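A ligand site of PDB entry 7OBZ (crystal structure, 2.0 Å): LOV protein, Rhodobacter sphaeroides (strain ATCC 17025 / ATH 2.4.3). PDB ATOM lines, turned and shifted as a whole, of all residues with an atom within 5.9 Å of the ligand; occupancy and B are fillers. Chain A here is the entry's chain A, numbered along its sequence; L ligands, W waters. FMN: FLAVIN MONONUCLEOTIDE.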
ATOM      1  N   THR A  21       1.047  19.761   7.786  1.00  0.00           N
ATOM      2  CA  THR A  21       1.655  20.719   8.695  1.00  0.00           C
ATOM      3  C   THR A  21       0.594  21.243   9.648  1.00  0.00           C
ATOM      4  O   THR A  21      -0.595  21.327   9.301  1.00  0.00           O
ATOM      5  CB  THR A  21       2.300  21.901   7.927  1.00  0.00           C
ATOM      6  OG1 THR A  21       1.328  22.510   7.068  1.00  0.00           O
ATOM      7  CG2 THR A  21       3.468  21.416   7.101  1.00  0.00           C
ATOM      8  N   LEU A  22       1.049  21.593  10.849  1.00  0.00           N
ATOM      9  CA  LEU A  22       0.223  22.194  11.885  1.00  0.00           C
ATOM     10  C   LEU A  22       0.888  23.475  12.356  1.00  0.00           C
ATOM     11  O   LEU A  22       2.077  23.478  12.685  1.00  0.00           O
ATOM     12  CB  LEU A  22       0.016  21.235  13.064  1.00  0.00           C
ATOM     13  CG  LEU A  22      -1.206  21.598  13.926  1.00  0.00           C
ATOM     14  CD1 LEU A  22      -2.546  21.335  13.198  1.00  0.00           C
ATOM     15  CD2 LEU A  22      -1.208  20.895  15.287  1.00  0.00           C
ATOM     16  N   VAL A  23       0.099  24.545  12.451  1.00  0.00           N
ATOM     17  CA  VAL A  23       0.594  25.872  12.804  1.00  0.00           C
ATOM     18  C   VAL A  23      -0.172  26.351  14.031  1.00  0.00           C
ATOM     19  O   VAL A  23      -1.406  26.238  14.085  1.00  0.00           O
ATOM     20  CB  VAL A  23       0.437  26.844  11.616  1.00  0.00           C
ATOM     21  CG1 VAL A  23       0.477  28.274  12.071  1.00  0.00           C
ATOM     22  CG2 VAL A  23       1.506  26.600  10.549  1.00  0.00           C
ATOM     23  N   MET A  25      -1.876  28.905  16.122  1.00  0.00           N
ATOM     24  CA  MET A  25      -2.599  30.127  15.828  1.00  0.00           C
ATOM     25  C   MET A  25      -2.656  31.086  17.014  1.00  0.00           C
ATOM     26  O   MET A  25      -3.136  32.208  16.872  1.00  0.00           O
ATOM     27  CB  MET A  25      -4.010  29.752  15.417  1.00  0.00           C
ATOM     28  CG  MET A  25      -4.199  29.383  13.964  1.00  0.00           C
ATOM     29  SD  MET A  25      -3.290  30.204  12.649  1.00  0.00           S
ATOM     30  CE  MET A  25      -4.418  31.540  12.254  1.00  0.00           C
ATOM     31  N   GLN A  30       2.630  32.758  14.091  1.00  0.00           N
ATOM     32  CA  GLN A  30       2.053  31.566  13.481  1.00  0.00           C
ATOM     33  C   GLN A  30       3.098  30.543  13.032  1.00  0.00           C
ATOM     34  O   GLN A  30       3.202  30.222  11.843  1.00  0.00           O
ATOM     35  CB  GLN A  30       1.162  31.962  12.307  1.00  0.00           C
ATOM     36  CG  GLN A  30      -0.104  32.718  12.730  1.00  0.00           C
ATOM     37  CD  GLN A  30      -0.872  33.283  11.552  1.00  0.00           C
ATOM     38  OE1 GLN A  30      -0.458  33.122  10.399  1.00  0.00           O
ATOM     39  NE2 GLN A  30      -1.981  33.940  11.831  1.00  0.00           N
ATOM     40  N   LEU A  32       5.117  26.884  12.496  1.00  0.00           N
ATOM     41  CA  LEU A  32       5.021  25.433  12.385  1.00  0.00           C
ATOM     42  C   LEU A  32       5.318  24.780  13.714  1.00  0.00           C
ATOM     43  O   LEU A  32       6.415  24.975  14.273  1.00  0.00           O
ATOM     44  CB  LEU A  32       6.030  24.928  11.351  1.00  0.00           C
ATOM     45  CG  LEU A  32       5.575  24.881   9.906  1.00  0.00           C
ATOM     46  CD1 LEU A  32       6.750  24.646   8.938  1.00  0.00           C
ATOM     47  CD2 LEU A  32       4.488  23.810   9.764  1.00  0.00           C
ATOM     48  N   PHE A  39       5.866  15.945   3.971  1.00  0.00           N
ATOM     49  CA  PHE A  39       6.151  17.358   3.812  1.00  0.00           C
ATOM     50  C   PHE A  39       7.658  17.613   3.785  1.00  0.00           C
ATOM     51  O   PHE A  39       8.152  18.382   2.942  1.00  0.00           O
ATOM     52  CB  PHE A  39       5.515  18.164   4.946  1.00  0.00           C
ATOM     53  CG  PHE A  39       5.873  19.635   4.895  1.00  0.00           C
ATOM     54  CD1 PHE A  39       5.119  20.507   4.127  1.00  0.00           C
ATOM     55  CD2 PHE A  39       6.992  20.126   5.581  1.00  0.00           C
ATOM     56  CE1 PHE A  39       5.425  21.850   4.077  1.00  0.00           C
ATOM     57  CE2 PHE A  39       7.329  21.476   5.519  1.00  0.00           C
ATOM     58  CZ  PHE A  39       6.555  22.343   4.764  1.00  0.00           C
ATOM     59  N   ASN A  54       7.464  30.388  10.560  1.00  0.00           N
ATOM     60  CA  ASN A  54       6.302  30.514   9.717  1.00  0.00           C
ATOM     61  C   ASN A  54       6.556  29.837   8.372  1.00  0.00           C
ATOM     62  O   ASN A  54       7.654  29.938   7.828  1.00  0.00           O
ATOM     63  CB  ASN A  54       5.957  31.979   9.510  1.00  0.00           C
ATOM     64  CG  ASN A  54       4.616  32.169   8.810  1.00  0.00           C
ATOM     65  OD1 ASN A  54       4.512  31.986   7.590  1.00  0.00           O
ATOM     66  ND2 ASN A  54       3.606  32.574   9.564  1.00  0.00           N
ATOM     67  N   CYS A  55       5.517  29.197   7.823  1.00  0.00           N
ATOM     68  CA  CYS A  55       5.618  28.451   6.576  1.00  0.00           C
ATOM     69  C   CYS A  55       5.966  29.306   5.374  1.00  0.00           C
ATOM     70  O   CYS A  55       6.317  28.754   4.314  1.00  0.00           O
ATOM     71  CB  CYS A  55       4.287  27.722   6.309  1.00  0.00           C
ATOM     72  SG  CYS A  55       3.952  26.372   7.470  1.00  0.00           S
ATOM     73  N   ARG A  56       5.878  30.623   5.477  1.00  0.00           N
ATOM     74  CA  ARG A  56       6.256  31.467   4.341  1.00  0.00           C
ATOM     75  C   ARG A  56       7.733  31.348   3.941  1.00  0.00           C
ATOM     76  O   ARG A  56       8.135  31.941   2.928  1.00  0.00           O
ATOM     77  CB  ARG A  56       5.925  32.924   4.666  1.00  0.00           C
ATOM     78  CG  ARG A  56       6.869  33.553   5.656  1.00  0.00           C
ATOM     79  CD  ARG A  56       6.740  35.054   5.688  1.00  0.00           C
ATOM     80  NE  ARG A  56       5.457  35.489   6.204  1.00  0.00           N
ATOM     81  CZ  ARG A  56       5.111  35.476   7.487  1.00  0.00           C
ATOM     82  NH1 ARG A  56       5.953  35.042   8.417  1.00  0.00           N
ATOM     83  NH2 ARG A  56       3.887  35.875   7.838  1.00  0.00           N
ATOM     84  N   LEU A  58       8.992  28.971   2.547  1.00  0.00           N
ATOM     85  CA  LEU A  58       8.985  28.248   1.285  1.00  0.00           C
ATOM     86  C   LEU A  58       8.894  29.162   0.089  1.00  0.00           C
ATOM     87  O   LEU A  58       9.121  28.707  -1.038  1.00  0.00           O
ATOM     88  CB  LEU A  58       7.807  27.269   1.255  1.00  0.00           C
ATOM     89  CG  LEU A  58       7.980  26.017   2.119  1.00  0.00           C
ATOM     90  CD1 LEU A  58       6.691  25.137   2.143  1.00  0.00           C
ATOM     91  CD2 LEU A  58       9.183  25.229   1.651  1.00  0.00           C
ATOM     92  N   GLN A  59       8.555  30.429   0.299  1.00  0.00           N
ATOM     93  CA  GLN A  59       8.423  31.435  -0.753  1.00  0.00           C
ATOM     94  C   GLN A  59       9.652  32.350  -0.789  1.00  0.00           C
ATOM     95  O   GLN A  59      10.446  32.393   0.160  1.00  0.00           O
ATOM     96  CB  GLN A  59       7.167  32.279  -0.524  1.00  0.00           C
ATOM     97  CG  GLN A  59       5.920  31.434  -0.286  1.00  0.00           C
ATOM     98  CD  GLN A  59       4.730  32.260   0.146  1.00  0.00           C
ATOM     99  OE1 GLN A  59       4.368  33.197  -0.536  1.00  0.00           O
ATOM    100  NE2 GLN A  59       4.125  31.908   1.288  1.00  0.00           N
ATOM    101  N   ASN A  64       3.290  35.580  -4.921  1.00  0.00           N
ATOM    102  CA  ASN A  64       2.016  35.070  -4.390  1.00  0.00           C
ATOM    103  C   ASN A  64       1.248  36.155  -3.621  1.00  0.00           C
ATOM    104  O   ASN A  64       0.490  35.842  -2.687  1.00  0.00           O
ATOM    105  CB  ASN A  64       2.225  33.829  -3.496  1.00  0.00           C
ATOM    106  CG  ASN A  64       3.227  32.840  -4.070  1.00  0.00           C
ATOM    107  OD1 ASN A  64       3.023  32.281  -5.136  1.00  0.00           O
ATOM    108  ND2 ASN A  64       4.316  32.618  -3.343  1.00  0.00           N
ATOM    109  N   ARG A  68      -1.532  35.202  -1.115  1.00  0.00           N
ATOM    110  CA  ARG A  68      -1.162  35.438   0.283  1.00  0.00           C
ATOM    111  C   ARG A  68      -2.219  36.287   0.985  1.00  0.00           C
ATOM    112  O   ARG A  68      -2.534  36.051   2.157  1.00  0.00           O
ATOM    113  CB  ARG A  68       0.237  36.101   0.358  1.00  0.00           C
ATOM    114  CG  ARG A  68       1.406  35.129   0.042  1.00  0.00           C
ATOM    115  CD  ARG A  68       2.817  35.684   0.383  1.00  0.00           C
ATOM    116  NE  ARG A  68       2.798  37.051   0.887  1.00  0.00           N
ATOM    117  CZ  ARG A  68       3.083  38.132   0.184  1.00  0.00           C
ATOM    118  NH1 ARG A  68       3.502  38.054  -1.084  1.00  0.00           N
ATOM    119  NH2 ARG A  68       2.930  39.323   0.741  1.00  0.00           N
ATOM    120  N   ALA A  69      -2.742  37.293   0.298  1.00  0.00           N
ATOM    121  CA  ALA A  69      -3.843  38.060   0.865  1.00  0.00           C
ATOM    122  C   ALA A  69      -5.068  37.169   1.099  1.00  0.00           C
ATOM    123  O   ALA A  69      -5.798  37.354   2.083  1.00  0.00           O
ATOM    124  CB  ALA A  69      -4.204  39.211  -0.057  1.00  0.00           C
ATOM    125  N   ILE A  71      -4.914  33.959   1.830  1.00  0.00           N
ATOM    126  CA  ILE A  71      -4.569  33.150   2.996  1.00  0.00           C
ATOM    127  C   ILE A  71      -4.767  33.947   4.278  1.00  0.00           C
ATOM    128  O   ILE A  71      -5.368  33.456   5.240  1.00  0.00           O
ATOM    129  CB  ILE A  71      -3.137  32.610   2.875  1.00  0.00           C
ATOM    130  CG1 ILE A  71      -3.042  31.618   1.720  1.00  0.00           C
ATOM    131  CG2 ILE A  71      -2.704  31.959   4.169  1.00  0.00           C
ATOM    132  CD1 ILE A  71      -1.623  31.335   1.236  1.00  0.00           C
ATOM    133  N   ARG A  72      -4.274  35.193   4.299  1.00  0.00           N
ATOM    134  CA  ARG A  72      -4.354  35.981   5.539  1.00  0.00           C
ATOM    135  C   ARG A  72      -5.803  36.189   5.974  1.00  0.00           C
ATOM    136  O   ARG A  72      -6.097  36.150   7.183  1.00  0.00           O
ATOM    137  CB  ARG A  72      -3.637  37.324   5.352  1.00  0.00           C
ATOM    138  CG  ARG A  72      -2.098  37.188   5.197  1.00  0.00           C
ATOM    139  CD  ARG A  72      -1.357  38.555   5.408  1.00  0.00           C
ATOM    140  NE  ARG A  72      -1.756  39.579   4.445  1.00  0.00           N
ATOM    141  CZ  ARG A  72      -1.314  39.653   3.187  1.00  0.00           C
ATOM    142  NH1 ARG A  72      -0.420  38.781   2.724  1.00  0.00           N
ATOM    143  NH2 ARG A  72      -1.811  40.579   2.384  1.00  0.00           N
ATOM    144  N   LEU A  75      -7.191  32.865   7.299  1.00  0.00           N
ATOM    145  CA  LEU A  75      -6.647  32.506   8.605  1.00  0.00           C
ATOM    146  C   LEU A  75      -7.296  33.335   9.695  1.00  0.00           C
ATOM    147  O   LEU A  75      -7.604  32.842  10.782  1.00  0.00           O
ATOM    148  CB  LEU A  75      -5.126  32.731   8.644  1.00  0.00           C
ATOM    149  CG  LEU A  75      -4.241  31.817   7.792  1.00  0.00           C
ATOM    150  CD1 LEU A  75      -2.735  32.247   7.908  1.00  0.00           C
ATOM    151  CD2 LEU A  75      -4.495  30.357   8.160  1.00  0.00           C
ATOM    152  N   LEU A  85       0.449  28.034  -4.509  1.00  0.00           N
ATOM    153  CA  LEU A  85       1.584  28.925  -4.253  1.00  0.00           C
ATOM    154  C   LEU A  85       2.802  28.482  -5.049  1.00  0.00           C
ATOM    155  O   LEU A  85       3.077  27.284  -5.158  1.00  0.00           O
ATOM    156  CB  LEU A  85       1.952  28.945  -2.777  1.00  0.00           C
ATOM    157  CG  LEU A  85       0.880  29.430  -1.817  1.00  0.00           C
ATOM    158  CD1 LEU A  85       1.322  29.167  -0.406  1.00  0.00           C
ATOM    159  CD2 LEU A  85       0.635  30.913  -2.040  1.00  0.00           C
ATOM    160  N   ARG A  86       3.540  29.450  -5.592  1.00  0.00           N
ATOM    161  CA  ARG A  86       4.930  29.215  -5.973  1.00  0.00           C
ATOM    162  C   ARG A  86       5.797  29.027  -4.729  1.00  0.00           C
ATOM    163  O   ARG A  86       5.796  29.863  -3.826  1.00  0.00           O
ATOM    164  CB  ARG A  86       5.448  30.384  -6.812  1.00  0.00           C
ATOM    165  CG  ARG A  86       6.947  30.293  -7.190  1.00  0.00           C
ATOM    166  CD  ARG A  86       7.363  28.908  -7.697  1.00  0.00           C
ATOM    167  NE  ARG A  86       6.610  28.506  -8.880  1.00  0.00           N
ATOM    168  CZ  ARG A  86       6.760  29.036 -10.084  1.00  0.00           C
ATOM    169  NH1 ARG A  86       7.676  29.966 -10.324  1.00  0.00           N
ATOM    170  NH2 ARG A  86       5.981  28.615 -11.077  1.00  0.00           N
ATOM    171  N   ASN A  87       6.515  27.917  -4.672  1.00  0.00           N
ATOM    172  CA  ASN A  87       7.362  27.581  -3.531  1.00  0.00           C
ATOM    173  C   ASN A  87       8.696  27.071  -4.056  1.00  0.00           C
ATOM    174  O   ASN A  87       8.861  26.795  -5.242  1.00  0.00           O
ATOM    175  CB  ASN A  87       6.709  26.527  -2.633  1.00  0.00           C
ATOM    176  CG  ASN A  87       5.749  27.131  -1.613  1.00  0.00           C
ATOM    177  OD1 ASN A  87       5.167  26.427  -0.791  1.00  0.00           O
ATOM    178  ND2 ASN A  87       5.602  28.433  -1.675  1.00  0.00           N
ATOM    179  N   ASN A  97       2.607  24.609  -5.468  1.00  0.00           N
ATOM    180  CA  ASN A  97       2.098  23.947  -4.268  1.00  0.00           C
ATOM    181  C   ASN A  97       0.606  24.243  -4.208  1.00  0.00           C
ATOM    182  O   ASN A  97       0.214  25.389  -3.976  1.00  0.00           O
ATOM    183  CB  ASN A  97       2.841  24.464  -3.047  1.00  0.00           C
ATOM    184  CG  ASN A  97       2.353  23.893  -1.713  1.00  0.00           C
ATOM    185  OD1 ASN A  97       1.346  23.152  -1.626  1.00  0.00           O
ATOM    186  ND2 ASN A  97       3.093  24.249  -0.650  1.00  0.00           N
ATOM    187  N   LEU A  99      -2.021  24.209  -1.890  1.00  0.00           N
ATOM    188  CA  LEU A  99      -2.092  24.171  -0.433  1.00  0.00           C
ATOM    189  C   LEU A  99      -3.540  24.081   0.032  1.00  0.00           C
ATOM    190  O   LEU A  99      -4.378  24.882  -0.392  1.00  0.00           O
ATOM    191  CB  LEU A  99      -1.434  25.405   0.187  1.00  0.00           C
ATOM    192  CG  LEU A  99      -1.458  25.585   1.697  1.00  0.00           C
ATOM    193  CD1 LEU A  99      -0.589  24.544   2.442  1.00  0.00           C
ATOM    194  CD2 LEU A  99      -1.038  26.997   2.085  1.00  0.00           C
ATOM    195  N   LEU A 101      -5.810  24.496   3.371  1.00  0.00           N
ATOM    196  CA  LEU A 101      -5.813  25.032   4.737  1.00  0.00           C
ATOM    197  C   LEU A 101      -7.097  24.601   5.464  1.00  0.00           C
ATOM    198  O   LEU A 101      -8.186  24.743   4.909  1.00  0.00           O
ATOM    199  CB  LEU A 101      -5.708  26.559   4.712  1.00  0.00           C
ATOM    200  CG  LEU A 101      -4.289  27.075   4.338  1.00  0.00           C
ATOM    201  CD1 LEU A 101      -4.264  28.583   4.160  1.00  0.00           C
ATOM    202  CD2 LEU A 101      -3.249  26.651   5.380  1.00  0.00           C
ATOM    203  N   PHE A 114      -4.002  25.854  12.743  1.00  0.00           N
ATOM    204  CA  PHE A 114      -4.384  25.617  11.373  1.00  0.00           C
ATOM    205  C   PHE A 114      -3.619  24.411  10.847  1.00  0.00           C
ATOM    206  O   PHE A 114      -2.442  24.214  11.175  1.00  0.00           O
ATOM    207  CB  PHE A 114      -4.136  26.804  10.473  1.00  0.00           C
ATOM    208  CG  PHE A 114      -5.402  27.443   9.949  1.00  0.00           C
ATOM    209  CD1 PHE A 114      -6.052  28.437  10.658  1.00  0.00           C
ATOM    210  CD2 PHE A 114      -5.918  27.048   8.731  1.00  0.00           C
ATOM    211  CE1 PHE A 114      -7.185  29.037  10.144  1.00  0.00           C
ATOM    212  CE2 PHE A 114      -7.059  27.638   8.209  1.00  0.00           C
ATOM    213  CZ  PHE A 114      -7.697  28.629   8.926  1.00  0.00           C
ATOM    214  N   LEU A 115      -4.323  23.602  10.048  1.00  0.00           N
ATOM    215  CA  LEU A 115      -3.721  22.453   9.398  1.00  0.00           C
ATOM    216  C   LEU A 115      -3.453  22.854   7.963  1.00  0.00           C
ATOM    217  O   LEU A 115      -4.232  23.619   7.388  1.00  0.00           O
ATOM    218  CB  LEU A 115      -4.624  21.225   9.449  1.00  0.00           C
ATOM    219  CG  LEU A 115      -4.057  19.971   8.778  1.00  0.00           C
ATOM    220  CD1 LEU A 115      -4.478  18.721   9.555  1.00  0.00           C
ATOM    221  CD2 LEU A 115      -4.499  19.838   7.294  1.00  0.00           C
ATOM    222  N   GLY A 116      -2.345  22.382   7.416  1.00  0.00           N
ATOM    223  CA  GLY A 116      -2.014  22.641   6.033  1.00  0.00           C
ATOM    224  C   GLY A 116      -1.524  21.362   5.393  1.00  0.00           C
ATOM    225  O   GLY A 116      -0.907  20.525   6.053  1.00  0.00           O
ATOM    226  N   SER A 117      -1.836  21.198   4.117  1.00  0.00           N
ATOM    227  CA  SER A 117      -1.513  19.983   3.401  1.00  0.00           C
ATOM    228  C   SER A 117      -1.160  20.370   1.980  1.00  0.00           C
ATOM    229  O   SER A 117      -1.901  21.120   1.344  1.00  0.00           O
ATOM    230  CB  SER A 117      -2.710  18.987   3.413  1.00  0.00           C
ATOM    231  OG  SER A 117      -2.470  17.836   2.605  1.00  0.00           O
ATOM    232  N   GLN A 118      -0.057  19.826   1.477  1.00  0.00           N
ATOM    233  CA  GLN A 118       0.590  20.354   0.268  1.00  0.00           C
ATOM    234  C   GLN A 118       0.566  19.284  -0.814  1.00  0.00           C
ATOM    235  O   GLN A 118       1.050  18.168  -0.587  1.00  0.00           O
ATOM    236  CB  GLN A 118       2.027  20.812   0.585  1.00  0.00           C
ATOM    237  CG  GLN A 118       2.077  22.012   1.523  1.00  0.00           C
ATOM    238  CD  GLN A 118       1.983  21.611   2.997  1.00  0.00           C
ATOM    239  OE1 GLN A 118       1.981  20.431   3.344  1.00  0.00           O
ATOM    240  NE2 GLN A 118       1.911  22.617   3.862  1.00  0.00           N
HETATM  241  N1  FMN L   1       2.922  28.989   2.662  1.00  0.00           N
HETATM  242  C2  FMN L   1       3.703  28.437   1.665  1.00  0.00           C
HETATM  243  O2  FMN L   1       4.272  29.152   0.828  1.00  0.00           O
HETATM  244  N3  FMN L   1       3.833  27.066   1.601  1.00  0.00           N
HETATM  245  C4  FMN L   1       3.211  26.254   2.522  1.00  0.00           C
HETATM  246  O4  FMN L   1       3.378  25.036   2.413  1.00  0.00           O
HETATM  247  C4A FMN L   1       2.418  26.811   3.526  1.00  0.00           C
HETATM  248  N5  FMN L   1       1.779  26.025   4.460  1.00  0.00           N
HETATM  249  C5A FMN L   1       1.034  26.637   5.450  1.00  0.00           C
HETATM  250  C6  FMN L   1       0.386  25.847   6.369  1.00  0.00           C
HETATM  251  C7  FMN L   1      -0.394  26.393   7.374  1.00  0.00           C
HETATM  252  C7M FMN L   1      -1.032  25.464   8.369  1.00  0.00           C
HETATM  253  C8  FMN L   1      -0.547  27.773   7.451  1.00  0.00           C
HETATM  254  C8M FMN L   1      -1.396  28.321   8.565  1.00  0.00           C
HETATM  255  C9  FMN L   1       0.114  28.594   6.517  1.00  0.00           C
HETATM  256  C9A FMN L   1       0.892  28.018   5.499  1.00  0.00           C
HETATM  257  N10 FMN L   1       1.508  28.777   4.558  1.00  0.00           N
HETATM  258  C10 FMN L   1       2.277  28.186   3.582  1.00  0.00           C
HETATM  259  C1' FMN L   1       1.342  30.273   4.523  1.00  0.00           C
HETATM  260  C2' FMN L   1       2.330  31.168   5.203  1.00  0.00           C
HETATM  261  O2' FMN L   1       2.681  30.605   6.440  1.00  0.00           O
HETATM  262  C3' FMN L   1       1.594  32.509   5.343  1.00  0.00           C
HETATM  263  O3' FMN L   1       0.392  32.369   6.073  1.00  0.00           O
HETATM  264  C4' FMN L   1       1.247  33.126   3.977  1.00  0.00           C
HETATM  265  O4' FMN L   1       2.431  33.261   3.218  1.00  0.00           O
HETATM  266  C5' FMN L   1       0.522  34.475   4.068  1.00  0.00           C
HETATM  267  O5' FMN L   1       1.107  35.257   5.081  1.00  0.00           O
HETATM  268  P   FMN L   1       2.186  36.439   4.673  1.00  0.00           P
HETATM  269  O1P FMN L   1       2.273  37.353   5.863  1.00  0.00           O
HETATM  270  O2P FMN L   1       3.443  35.699   4.335  1.00  0.00           O
HETATM  271  O3P FMN L   1       1.773  37.169   3.420  1.00  0.00           O
HETATM  272  O   HOH W   1       5.406  36.471   2.294  1.00  0.00           O
HETATM  273  O   HOH W   2      -0.017  34.265   7.500  1.00  0.00           O
HETATM  274  O   HOH W   3       4.496  38.856   6.106  1.00  0.00           O
HETATM  275  O   HOH W   4       2.712  29.270   9.140  1.00  0.00           O
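The backbone NH (N) of Cys 55 lies close to an oxygen (O2') of the ligand (3.5 Å).
O2P of the ligand is in salt-bridge range of NE of Arg 56.
NE2 of Gln 59 lies within hydrogen-bond range of O2 of the ligand, at 2.8 Å.
O2' of the ligand lies within hydrogen-bond range of OD1 of Asn 54, at 2.6 Å.
The side-chain amide nitrogen (ND2) of Asn 97 sits at hydrogen-bond distance from an oxygen (O4) of the ligand.
SG of Cys 55 sits close to N5 of the ligand, 3.7 Å away.
The backbone NH of Arg 56 sits at hydrogen-bond distance from an oxygen (O2') of the ligand, 3.3 Å away.
An oxygen (O4) of the ligand is in hydrogen-bond range of the side-chain amide nitrogen of Gln 118 (3.2 Å).
OD1 of Asn 87 is in hydrogen-bond range of N3 of the ligand.
NE of Arg 68 lies within salt-bridge range of O3P of the ligand (2.7 Å).
The guanidinium group (NH1) of Arg 72 is in salt-bridge range of an oxygen (O3P) of the ligand, 2.8 Å away.
Residues that only touch the ligand: Thr 21 (3.5 Å), Val 23 (3.5 Å), Leu 58 (3.3 Å), Ile 71 (3.7 Å), Leu 75 (3.6 Å), Leu 85 (3.2 Å), Leu 99 (3.4 Å), Leu 101 (3.5 Å), Phe 114 (3.4 Å), Leu 115 (3.6 Å) and Gly 116 (3.5 Å).
20 residues have an atom within 4 Å of the ligand: Thr 21, Val 23, Asn 54, Cys 55, Arg 56, Leu 58, Gln 59, Arg 68, Ile 71, Arg 72, Leu 75, Leu 85, Asn 87, Asn 97, Leu 99, Leu 101, Phe 114, Leu 115, Gly 116 and Gln 118.
The nearest printed residue that does not touch the ligand is Phe 39 (4.1 Å).
OD1 of Asn 54 is in hydrogen-bond range of N of Arg 56, at 2.9 Å.
The side-chain amide oxygen (OD1) of Asn 87 is in hydrogen-bond range of the side-chain amide nitrogen (ND2) of Asn 97 (3.0 Å).
O of Arg 68 lies close to NH1 of Arg 72 (3.5 Å).
O of Gly 116 sits at hydrogen-bond distance from N of Thr 21 (2.7 Å).
ND2 of Asn 64 lies within hydrogen-bond range of OE1 of Gln 59.
N of Val 23 sits at hydrogen-bond distance from O of Phe 114 (2.9 Å).
O of Asn 97 is in hydrogen-bond range of N of Leu 85.
The side-chain amide nitrogen (ND2) of Asn 54 sits at hydrogen-bond distance from the backbone carbonyl oxygen (O) of Gln 30 (3.3 Å).
Water W2 bridges O3' of the ligand (2.4 Å) and OE1 of Gln 30 (3.1 Å).
Water W1 lies within hydrogen-bond range of an oxygen (O2P) of the ligand (2.9 Å) and the guanidinium group of Arg 68 (3.0 Å).
Water W4 lies within hydrogen-bond range of O of Gln 30 (2.9 Å), O2' of the ligand (3.0 Å), N of Cys 55 (3.1 Å) and ND2 of Asn 54 (3.4 Å).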
